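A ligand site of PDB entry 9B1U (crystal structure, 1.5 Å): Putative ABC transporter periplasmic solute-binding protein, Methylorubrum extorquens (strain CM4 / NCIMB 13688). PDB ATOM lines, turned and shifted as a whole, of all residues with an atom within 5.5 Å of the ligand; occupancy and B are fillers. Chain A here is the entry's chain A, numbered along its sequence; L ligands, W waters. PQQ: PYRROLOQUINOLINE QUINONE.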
ATOM      1  N   GLY A   8      25.732 -17.725  20.568  1.00  0.00           N
ATOM      2  CA  GLY A   8      24.644 -17.914  19.604  1.00  0.00           C
ATOM      3  C   GLY A   8      24.453 -19.382  19.275  1.00  0.00           C
ATOM      4  O   GLY A   8      25.447 -20.038  18.972  1.00  0.00           O
ATOM      5  N   VAL A   9      23.215 -19.845  19.356  1.00  0.00           N
ATOM      6  CA  VAL A   9      22.930 -21.296  19.133  1.00  0.00           C
ATOM      7  C   VAL A   9      21.779 -21.487  18.137  1.00  0.00           C
ATOM      8  O   VAL A   9      20.873 -20.668  18.120  1.00  0.00           O
ATOM      9  CB  VAL A   9      22.615 -22.019  20.454  1.00  0.00           C
ATOM     10  CG1 VAL A   9      23.780 -21.952  21.428  1.00  0.00           C
ATOM     11  CG2 VAL A   9      21.334 -21.509  21.094  1.00  0.00           C
ATOM     12  N   LEU A  10      21.828 -22.587  17.396  1.00  0.00           N
ATOM     13  CA  LEU A  10      20.760 -22.928  16.440  1.00  0.00           C
ATOM     14  C   LEU A  10      19.718 -23.809  17.136  1.00  0.00           C
ATOM     15  O   LEU A  10      20.066 -24.615  17.981  1.00  0.00           O
ATOM     16  CB  LEU A  10      21.387 -23.676  15.270  1.00  0.00           C
ATOM     17  CG  LEU A  10      22.456 -22.925  14.471  1.00  0.00           C
ATOM     18  CD1 LEU A  10      22.850 -23.717  13.237  1.00  0.00           C
ATOM     19  CD2 LEU A  10      21.960 -21.541  14.077  1.00  0.00           C
ATOM     20  N   PHE A  12      18.102 -26.398  16.077  1.00  0.00           N
ATOM     21  CA  PHE A  12      18.243 -27.832  15.728  1.00  0.00           C
ATOM     22  C   PHE A  12      19.680 -28.275  15.982  1.00  0.00           C
ATOM     23  O   PHE A  12      20.022 -29.389  15.648  1.00  0.00           O
ATOM     24  CB  PHE A  12      17.831 -27.992  14.264  1.00  0.00           C
ATOM     25  CG  PHE A  12      18.555 -27.115  13.285  1.00  0.00           C
ATOM     26  CD1 PHE A  12      19.811 -27.454  12.827  1.00  0.00           C
ATOM     27  CD2 PHE A  12      17.995 -25.925  12.847  1.00  0.00           C
ATOM     28  CE1 PHE A  12      20.474 -26.636  11.929  1.00  0.00           C
ATOM     29  CE2 PHE A  12      18.666 -25.108  11.959  1.00  0.00           C
ATOM     30  CZ  PHE A  12      19.908 -25.466  11.503  1.00  0.00           C
ATOM     31  N   GLY A  13      20.458 -27.390  16.591  1.00  0.00           N
ATOM     32  CA  GLY A  13      21.860 -27.714  16.857  1.00  0.00           C
ATOM     33  C   GLY A  13      22.082 -28.469  18.161  1.00  0.00           C
ATOM     34  O   GLY A  13      21.168 -28.545  18.973  1.00  0.00           O
ATOM     35  N   THR A  14      23.302 -28.993  18.329  1.00  0.00           N
ATOM     36  CA  THR A  14      23.662 -29.754  19.565  1.00  0.00           C
ATOM     37  C   THR A  14      24.351 -28.866  20.623  1.00  0.00           C
ATOM     38  O   THR A  14      24.470 -29.323  21.728  1.00  0.00           O
ATOM     39  CB  THR A  14      24.522 -30.964  19.184  1.00  0.00           C
ATOM     40  OG1 THR A  14      25.818 -30.556  18.774  1.00  0.00           O
ATOM     41  CG2 THR A  14      23.888 -31.790  18.085  1.00  0.00           C
ATOM     42  N   ALA A  15      24.773 -27.653  20.259  1.00  0.00           N
ATOM     43  CA  ALA A  15      25.510 -26.783  21.219  1.00  0.00           C
ATOM     44  C   ALA A  15      24.604 -26.439  22.387  1.00  0.00           C
ATOM     45  O   ALA A  15      25.097 -26.317  23.497  1.00  0.00           O
ATOM     46  CB  ALA A  15      25.996 -25.547  20.533  1.00  0.00           C
ATOM     47  N   SER A  16      23.301 -26.339  22.131  1.00  0.00           N
ATOM     48  CA  SER A  16      22.330 -26.035  23.206  1.00  0.00           C
ATOM     49  C   SER A  16      22.373 -27.096  24.320  1.00  0.00           C
ATOM     50  O   SER A  16      22.123 -26.754  25.472  1.00  0.00           O
ATOM     51  CB  SER A  16      20.947 -25.940  22.612  1.00  0.00           C
ATOM     52  OG  SER A  16      20.853 -24.814  21.768  1.00  0.00           O
ATOM     53  N   ASN A  43      21.683 -20.661  10.337  1.00  0.00           N
ATOM     54  CA  ASN A  43      23.129 -20.380  10.219  1.00  0.00           C
ATOM     55  C   ASN A  43      23.381 -19.031   9.552  1.00  0.00           C
ATOM     56  O   ASN A  43      24.315 -18.356   9.925  1.00  0.00           O
ATOM     57  CB  ASN A  43      23.822 -21.522   9.486  1.00  0.00           C
ATOM     58  CG  ASN A  43      25.198 -21.769  10.020  1.00  0.00           C
ATOM     59  OD1 ASN A  43      25.396 -21.737  11.227  1.00  0.00           O
ATOM     60  ND2 ASN A  43      26.160 -21.953   9.141  1.00  0.00           N
ATOM     61  N   VAL A  59      28.791 -21.544  16.908  1.00  0.00           N
ATOM     62  CA  VAL A  59      29.404 -22.828  16.499  1.00  0.00           C
ATOM     63  C   VAL A  59      29.448 -22.822  14.969  1.00  0.00           C
ATOM     64  O   VAL A  59      28.485 -22.383  14.358  1.00  0.00           O
ATOM     65  CB  VAL A  59      28.662 -24.042  17.077  1.00  0.00           C
ATOM     66  CG1 VAL A  59      29.207 -25.349  16.533  1.00  0.00           C
ATOM     67  CG2 VAL A  59      28.710 -24.031  18.590  1.00  0.00           C
ATOM     68  N   GLY A  60      30.537 -23.257  14.396  1.00  0.00           N
ATOM     69  CA  GLY A  60      30.601 -23.283  12.949  1.00  0.00           C
ATOM     70  C   GLY A  60      31.697 -24.198  12.467  1.00  0.00           C
ATOM     71  O   GLY A  60      32.277 -24.902  13.281  1.00  0.00           O
ATOM     72  N   ASP A  61      31.983 -24.110  11.190  1.00  0.00           N
ATOM     73  CA  ASP A  61      32.963 -25.052  10.627  1.00  0.00           C
ATOM     74  C   ASP A  61      34.309 -24.348  10.371  1.00  0.00           C
ATOM     75  O   ASP A  61      34.344 -23.132  10.264  1.00  0.00           O
ATOM     76  CB  ASP A  61      32.382 -25.783   9.429  1.00  0.00           C
ATOM     77  CG  ASP A  61      32.196 -24.881   8.242  1.00  0.00           C
ATOM     78  OD1 ASP A  61      33.178 -24.665   7.524  1.00  0.00           O
ATOM     79  OD2 ASP A  61      31.090 -24.370   8.077  1.00  0.00           O
ATOM     80  N   TYR A  80      34.949 -28.319  18.545  1.00  0.00           N
ATOM     81  CA  TYR A  80      33.671 -28.568  19.247  1.00  0.00           C
ATOM     82  C   TYR A  80      33.339 -30.057  19.120  1.00  0.00           C
ATOM     83  O   TYR A  80      32.963 -30.652  20.117  1.00  0.00           O
ATOM     84  CB  TYR A  80      32.563 -27.683  18.666  1.00  0.00           C
ATOM     85  CG  TYR A  80      31.181 -28.098  19.149  1.00  0.00           C
ATOM     86  CD1 TYR A  80      30.706 -27.704  20.392  1.00  0.00           C
ATOM     87  CD2 TYR A  80      30.379 -28.934  18.381  1.00  0.00           C
ATOM     88  CE1 TYR A  80      29.455 -28.086  20.840  1.00  0.00           C
ATOM     89  CE2 TYR A  80      29.134 -29.332  18.824  1.00  0.00           C
ATOM     90  CZ  TYR A  80      28.678 -28.912  20.053  1.00  0.00           C
ATOM     91  OH  TYR A  80      27.460 -29.320  20.484  1.00  0.00           O
ATOM     92  N   THR A  83      32.386 -35.332  15.274  1.00  0.00           N
ATOM     93  CA  THR A  83      31.220 -35.958  14.599  1.00  0.00           C
ATOM     94  C   THR A  83      30.621 -34.910  13.655  1.00  0.00           C
ATOM     95  O   THR A  83      30.240 -33.848  14.115  1.00  0.00           O
ATOM     96  CB  THR A  83      30.220 -36.517  15.615  1.00  0.00           C
ATOM     97  OG1 THR A  83      30.900 -37.469  16.429  1.00  0.00           O
ATOM     98  CG2 THR A  83      29.022 -37.173  14.972  1.00  0.00           C
ATOM     99  N   GLU A  84      30.595 -35.223  12.366  1.00  0.00           N
ATOM    100  CA  GLU A  84      30.096 -34.230  11.399  1.00  0.00           C
ATOM    101  C   GLU A  84      29.497 -34.904  10.163  1.00  0.00           C
ATOM    102  O   GLU A  84      30.140 -35.801   9.615  1.00  0.00           O
ATOM    103  CB  GLU A  84      31.183 -33.261  10.929  1.00  0.00           C
ATOM    104  CG  GLU A  84      32.519 -33.906  10.625  1.00  0.00           C
ATOM    105  CD  GLU A  84      33.692 -33.567  11.519  1.00  0.00           C
ATOM    106  OE1 GLU A  84      33.564 -32.706  12.405  1.00  0.00           O
ATOM    107  OE2 GLU A  84      34.740 -34.186  11.346  1.00  0.00           O
ATOM    108  N   GLY A  85      28.305 -34.475   9.786  1.00  0.00           N
ATOM    109  CA  GLY A  85      27.719 -34.834   8.485  1.00  0.00           C
ATOM    110  C   GLY A  85      27.114 -36.216   8.443  1.00  0.00           C
ATOM    111  O   GLY A  85      27.563 -37.112   9.157  1.00  0.00           O
ATOM    112  N   ASP A 114      29.021 -25.452   1.812  1.00  0.00           N
ATOM    113  CA  ASP A 114      28.993 -26.226   3.073  1.00  0.00           C
ATOM    114  C   ASP A 114      30.177 -27.193   3.153  1.00  0.00           C
ATOM    115  O   ASP A 114      30.445 -27.903   2.202  1.00  0.00           O
ATOM    116  CB  ASP A 114      27.688 -26.993   3.297  1.00  0.00           C
ATOM    117  CG  ASP A 114      27.669 -27.780   4.588  1.00  0.00           C
ATOM    118  OD1 ASP A 114      27.396 -27.185   5.639  1.00  0.00           O
ATOM    119  OD2 ASP A 114      27.943 -28.983   4.533  1.00  0.00           O
ATOM    120  N   LYS A 115      30.782 -27.265   4.334  1.00  0.00           N
ATOM    121  CA  LYS A 115      31.991 -28.101   4.503  1.00  0.00           C
ATOM    122  C   LYS A 115      31.726 -29.574   4.194  1.00  0.00           C
ATOM    123  O   LYS A 115      32.615 -30.197   3.662  1.00  0.00           O
ATOM    124  CB  LYS A 115      32.540 -27.923   5.926  1.00  0.00           C
ATOM    125  CG  LYS A 115      31.808 -28.641   7.047  1.00  0.00           C
ATOM    126  CD  LYS A 115      30.415 -28.133   7.338  1.00  0.00           C
ATOM    127  CE  LYS A 115      29.789 -28.801   8.539  1.00  0.00           C
ATOM    128  NZ  LYS A 115      28.355 -28.469   8.679  1.00  0.00           N
ATOM    129  N   ASN A 116      30.560 -30.092   4.549  1.00  0.00           N
ATOM    130  CA  ASN A 116      30.276 -31.529   4.325  1.00  0.00           C
ATOM    131  C   ASN A 116      30.137 -31.771   2.822  1.00  0.00           C
ATOM    132  O   ASN A 116      30.539 -32.829   2.355  1.00  0.00           O
ATOM    133  CB  ASN A 116      29.005 -31.970   5.043  1.00  0.00           C
ATOM    134  CG  ASN A 116      29.118 -31.931   6.553  1.00  0.00           C
ATOM    135  OD1 ASN A 116      30.207 -32.138   7.100  1.00  0.00           O
ATOM    136  ND2 ASN A 116      28.016 -31.666   7.229  1.00  0.00           N
ATOM    137  N   LEU A 160      23.101 -34.080   5.516  1.00  0.00           N
ATOM    138  CA  LEU A 160      22.583 -33.268   6.632  1.00  0.00           C
ATOM    139  C   LEU A 160      23.595 -33.216   7.775  1.00  0.00           C
ATOM    140  O   LEU A 160      24.639 -33.838   7.665  1.00  0.00           O
ATOM    141  CB  LEU A 160      21.322 -33.972   7.151  1.00  0.00           C
ATOM    142  CG  LEU A 160      20.192 -34.159   6.148  1.00  0.00           C
ATOM    143  CD1 LEU A 160      19.156 -35.130   6.687  1.00  0.00           C
ATOM    144  CD2 LEU A 160      19.536 -32.823   5.838  1.00  0.00           C
ATOM    145  N   TYR A 161      23.229 -32.483   8.809  1.00  0.00           N
ATOM    146  CA  TYR A 161      24.089 -32.482  10.012  1.00  0.00           C
ATOM    147  C   TYR A 161      23.909 -33.840  10.659  1.00  0.00           C
ATOM    148  O   TYR A 161      22.856 -34.473  10.519  1.00  0.00           O
ATOM    149  CB  TYR A 161      23.683 -31.318  10.918  1.00  0.00           C
ATOM    150  CG  TYR A 161      23.984 -29.913  10.437  1.00  0.00           C
ATOM    151  CD1 TYR A 161      24.531 -29.674   9.189  1.00  0.00           C
ATOM    152  CD2 TYR A 161      23.757 -28.817  11.260  1.00  0.00           C
ATOM    153  CE1 TYR A 161      24.808 -28.385   8.750  1.00  0.00           C
ATOM    154  CE2 TYR A 161      24.034 -27.527  10.839  1.00  0.00           C
ATOM    155  CZ  TYR A 161      24.561 -27.314   9.587  1.00  0.00           C
ATOM    156  OH  TYR A 161      24.841 -26.046   9.173  1.00  0.00           O
ATOM    157  N   TRP A 162      24.920 -34.247  11.412  1.00  0.00           N
ATOM    158  CA  TRP A 162      24.927 -35.615  12.007  1.00  0.00           C
ATOM    159  C   TRP A 162      23.703 -35.931  12.861  1.00  0.00           C
ATOM    160  O   TRP A 162      23.228 -37.066  12.805  1.00  0.00           O
ATOM    161  CB  TRP A 162      26.236 -35.819  12.778  1.00  0.00           C
ATOM    162  CG  TRP A 162      26.320 -35.152  14.119  1.00  0.00           C
ATOM    163  CD1 TRP A 162      26.981 -33.989  14.398  1.00  0.00           C
ATOM    164  CD2 TRP A 162      25.784 -35.628  15.364  1.00  0.00           C
ATOM    165  NE1 TRP A 162      26.874 -33.701  15.733  1.00  0.00           N
ATOM    166  CE2 TRP A 162      26.147 -34.694  16.349  1.00  0.00           C
ATOM    167  CE3 TRP A 162      25.035 -36.747  15.745  1.00  0.00           C
ATOM    168  CZ2 TRP A 162      25.781 -34.840  17.684  1.00  0.00           C
ATOM    169  CZ3 TRP A 162      24.674 -36.888  17.068  1.00  0.00           C
ATOM    170  CH2 TRP A 162      25.049 -35.950  18.018  1.00  0.00           C
ATOM    171  N   GLN A 163      23.187 -34.965  13.615  1.00  0.00           N
ATOM    172  CA  GLN A 163      22.091 -35.297  14.558  1.00  0.00           C
ATOM    173  C   GLN A 163      20.860 -35.786  13.784  1.00  0.00           C
ATOM    174  O   GLN A 163      20.023 -36.463  14.357  1.00  0.00           O
ATOM    175  CB  GLN A 163      21.766 -34.106  15.466  1.00  0.00           C
ATOM    176  CG  GLN A 163      21.438 -32.819  14.730  1.00  0.00           C
ATOM    177  CD  GLN A 163      22.635 -31.924  14.520  1.00  0.00           C
ATOM    178  OE1 GLN A 163      23.730 -32.385  14.226  1.00  0.00           O
ATOM    179  NE2 GLN A 163      22.428 -30.628  14.694  1.00  0.00           N
ATOM    180  N   ILE A 195      33.974 -29.028  13.129  1.00  0.00           N
ATOM    181  CA  ILE A 195      32.981 -28.161  13.824  1.00  0.00           C
ATOM    182  C   ILE A 195      33.650 -27.608  15.076  1.00  0.00           C
ATOM    183  O   ILE A 195      34.353 -28.363  15.762  1.00  0.00           O
ATOM    184  CB  ILE A 195      31.722 -28.960  14.198  1.00  0.00           C
ATOM    185  CG1 ILE A 195      31.243 -29.863  13.053  1.00  0.00           C
ATOM    186  CG2 ILE A 195      30.616 -28.024  14.679  1.00  0.00           C
ATOM    187  CD1 ILE A 195      30.862 -29.108  11.806  1.00  0.00           C
HETATM  188  N1  PQQ L   1      25.557 -26.787  15.552  1.00  0.00           N
HETATM  189  C2  PQQ L   1      25.362 -25.451  15.833  1.00  0.00           C
HETATM  190  C2X PQQ L   1      24.696 -25.016  17.034  1.00  0.00           C
HETATM  191  O2A PQQ L   1      24.317 -25.869  17.780  1.00  0.00           O
HETATM  192  O2B PQQ L   1      24.526 -23.827  17.178  1.00  0.00           O
HETATM  193  C3  PQQ L   1      25.867 -24.718  14.777  1.00  0.00           C
HETATM  194  C3A PQQ L   1      26.390 -25.605  13.833  1.00  0.00           C
HETATM  195  C1A PQQ L   1      26.223 -26.887  14.348  1.00  0.00           C
HETATM  196  C4  PQQ L   1      27.034 -25.400  12.554  1.00  0.00           C
HETATM  197  O4  PQQ L   1      27.307 -24.320  12.070  1.00  0.00           O
HETATM  198  C5  PQQ L   1      27.389 -26.645  11.747  1.00  0.00           C
HETATM  199  O5  PQQ L   1      27.951 -26.503  10.672  1.00  0.00           O
HETATM  200  C6A PQQ L   1      27.101 -27.960  12.309  1.00  0.00           C
HETATM  201  N6  PQQ L   1      27.392 -29.016  11.563  1.00  0.00           N
HETATM  202  C7  PQQ L   1      27.158 -30.223  12.024  1.00  0.00           C
HETATM  203  C7X PQQ L   1      27.491 -31.344  11.094  1.00  0.00           C
HETATM  204  O7A PQQ L   1      27.174 -32.486  11.433  1.00  0.00           O
HETATM  205  O7B PQQ L   1      28.004 -31.042  10.005  1.00  0.00           O
HETATM  206  C8  PQQ L   1      26.609 -30.452  13.300  1.00  0.00           C
HETATM  207  C9  PQQ L   1      26.292 -29.383  14.111  1.00  0.00           C
HETATM  208  C9X PQQ L   1      25.732 -29.662  15.483  1.00  0.00           C
HETATM  209  O9A PQQ L   1      24.666 -29.186  15.845  1.00  0.00           O
HETATM  210  O9B PQQ L   1      26.423 -30.386  16.196  1.00  0.00           O
HETATM  211  C9A PQQ L   1      26.570 -28.069  13.619  1.00  0.00           C
HETATM  212  O   HOH W   1      26.945 -25.567   7.562  1.00  0.00           O
HETATM  213  O   HOH W   2      22.245 -25.408  19.422  1.00  0.00           O
HETATM  214  O   HOH W   3      25.839 -21.489  16.654  1.00  0.00           O
HETATM  215  O   HOH W   4      28.932 -31.774  16.012  1.00  0.00           O
HETATM  216  O   HOH W   5      28.901 -24.357   9.407  1.00  0.00           O
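O9A of the ligand is in hydrogen-bond range of N of Thr 14, 2.8 Å away.
The side-chain hydroxyl (OG1) of Thr 14 lies within hydrogen-bond range of an oxygen (O9B) of the ligand (2.7 Å).
An oxygen (O7A) of the ligand is in hydrogen-bond range of the backbone NH of Gly 85, at 2.8 Å.
The side-chain amino group (NZ) of Lys 115 is in salt-bridge range of an oxygen (O7B) of the ligand, 2.9 Å away.
O7B of the ligand lies within hydrogen-bond range of ND2 of Asn 116 (2.8 Å).
N of Trp 162 is in hydrogen-bond range of O7A of the ligand (2.9 Å).
NE1 of Trp 162 is in hydrogen-bond range of O9B of the ligand (3.4 Å).
NE2 of Gln 163 sits at hydrogen-bond distance from O9A of the ligand (2.9 Å).
The backbone NH (N) of Leu 10 lies within hydrogen-bond range of an oxygen (O2B) of the ligand (3.0 Å).
The backbone NH (N) of Ala 15 lies within hydrogen-bond range of an oxygen (O2A) of the ligand, 3.1 Å away.
An oxygen (O4) of the ligand lies close to the side-chain amide oxygen (OD1) of Asn 43, 3.3 Å away.
OH of Tyr 161 is in hydrogen-bond range of O5 of the ligand (3.5 Å).
The side-chain hydroxyl of Thr 14 is in hydrogen-bond range of the side-chain hydroxyl of Tyr 80, 2.7 Å away.
NZ of Lys 115 is in salt-bridge range of OD1 of Asp 114, 3.4 Å away.
N of Asn 116 lies within hydrogen-bond range of OD2 of Asp 114.
The backbone carbonyl oxygen (O) of Phe 12 is in hydrogen-bond range of the side-chain amide nitrogen (NE2) of Gln 163.
OH of Tyr 80 lies within hydrogen-bond range of N of Ala 15 (3.2 Å).
The backbone carbonyl oxygen of Ile 195 lies within hydrogen-bond range of the backbone NH of Tyr 80, 2.8 Å away.
The backbone carbonyl oxygen (O) of Val 59 sits close to an oxygen (O4) of the ligand.
CA of Val 9 touches O2B of the ligand, 3.6 Å away.
Gly 13 touches the ligand.
CA of Gly 60 touches O4 of the ligand, at 3.6 Å.
Tyr 80 touches the ligand (CE2 to O9B, 3.9 Å).
CA of Glu 84 touches O7A of the ligand, 3.4 Å away.
Ile 195 touches the ligand.
Hydrophobic or aromatic side chains within 4 Å of the ligand: Leu 10, Ala 15, Val 59, Tyr 80, Tyr 161, Trp 162 and Ile 195.
Of the 24 residues printed, 17 come within 4 Å of the ligand.
Along chain A the residues within 4 Å of the ligand span positions 9 to 195.
Water W5 bridges OD2 of Asp 61 and O5 of the ligand.
Water W2 lies within hydrogen-bond range of an oxygen (O2A) of the ligand, the backbone carbonyl oxygen (O) of Leu 10, the side-chain hydroxyl (OG) of Ser 16, the backbone carbonyl oxygen (O) of Gly 13 and the backbone NH (N) of Ala 15.
Water W3 lies within hydrogen-bond range of O2B of the ligand, O of Gly 8 and N of Val 59.
Water W4 lies within hydrogen-bond range of NE1 of Trp 162 (2.8 Å), O9B of the ligand (2.9 Å) and O of Thr 83 (3.1 Å).
Water W1 lies within hydrogen-bond range of the side-chain carboxylate of Asp 114 (2.6 Å), the side-chain hydroxyl of Tyr 161 (2.7 Å), an oxygen (O5) of the ligand (3.4 Å) and the side-chain amino group of Lys 115 (3.4 Å).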
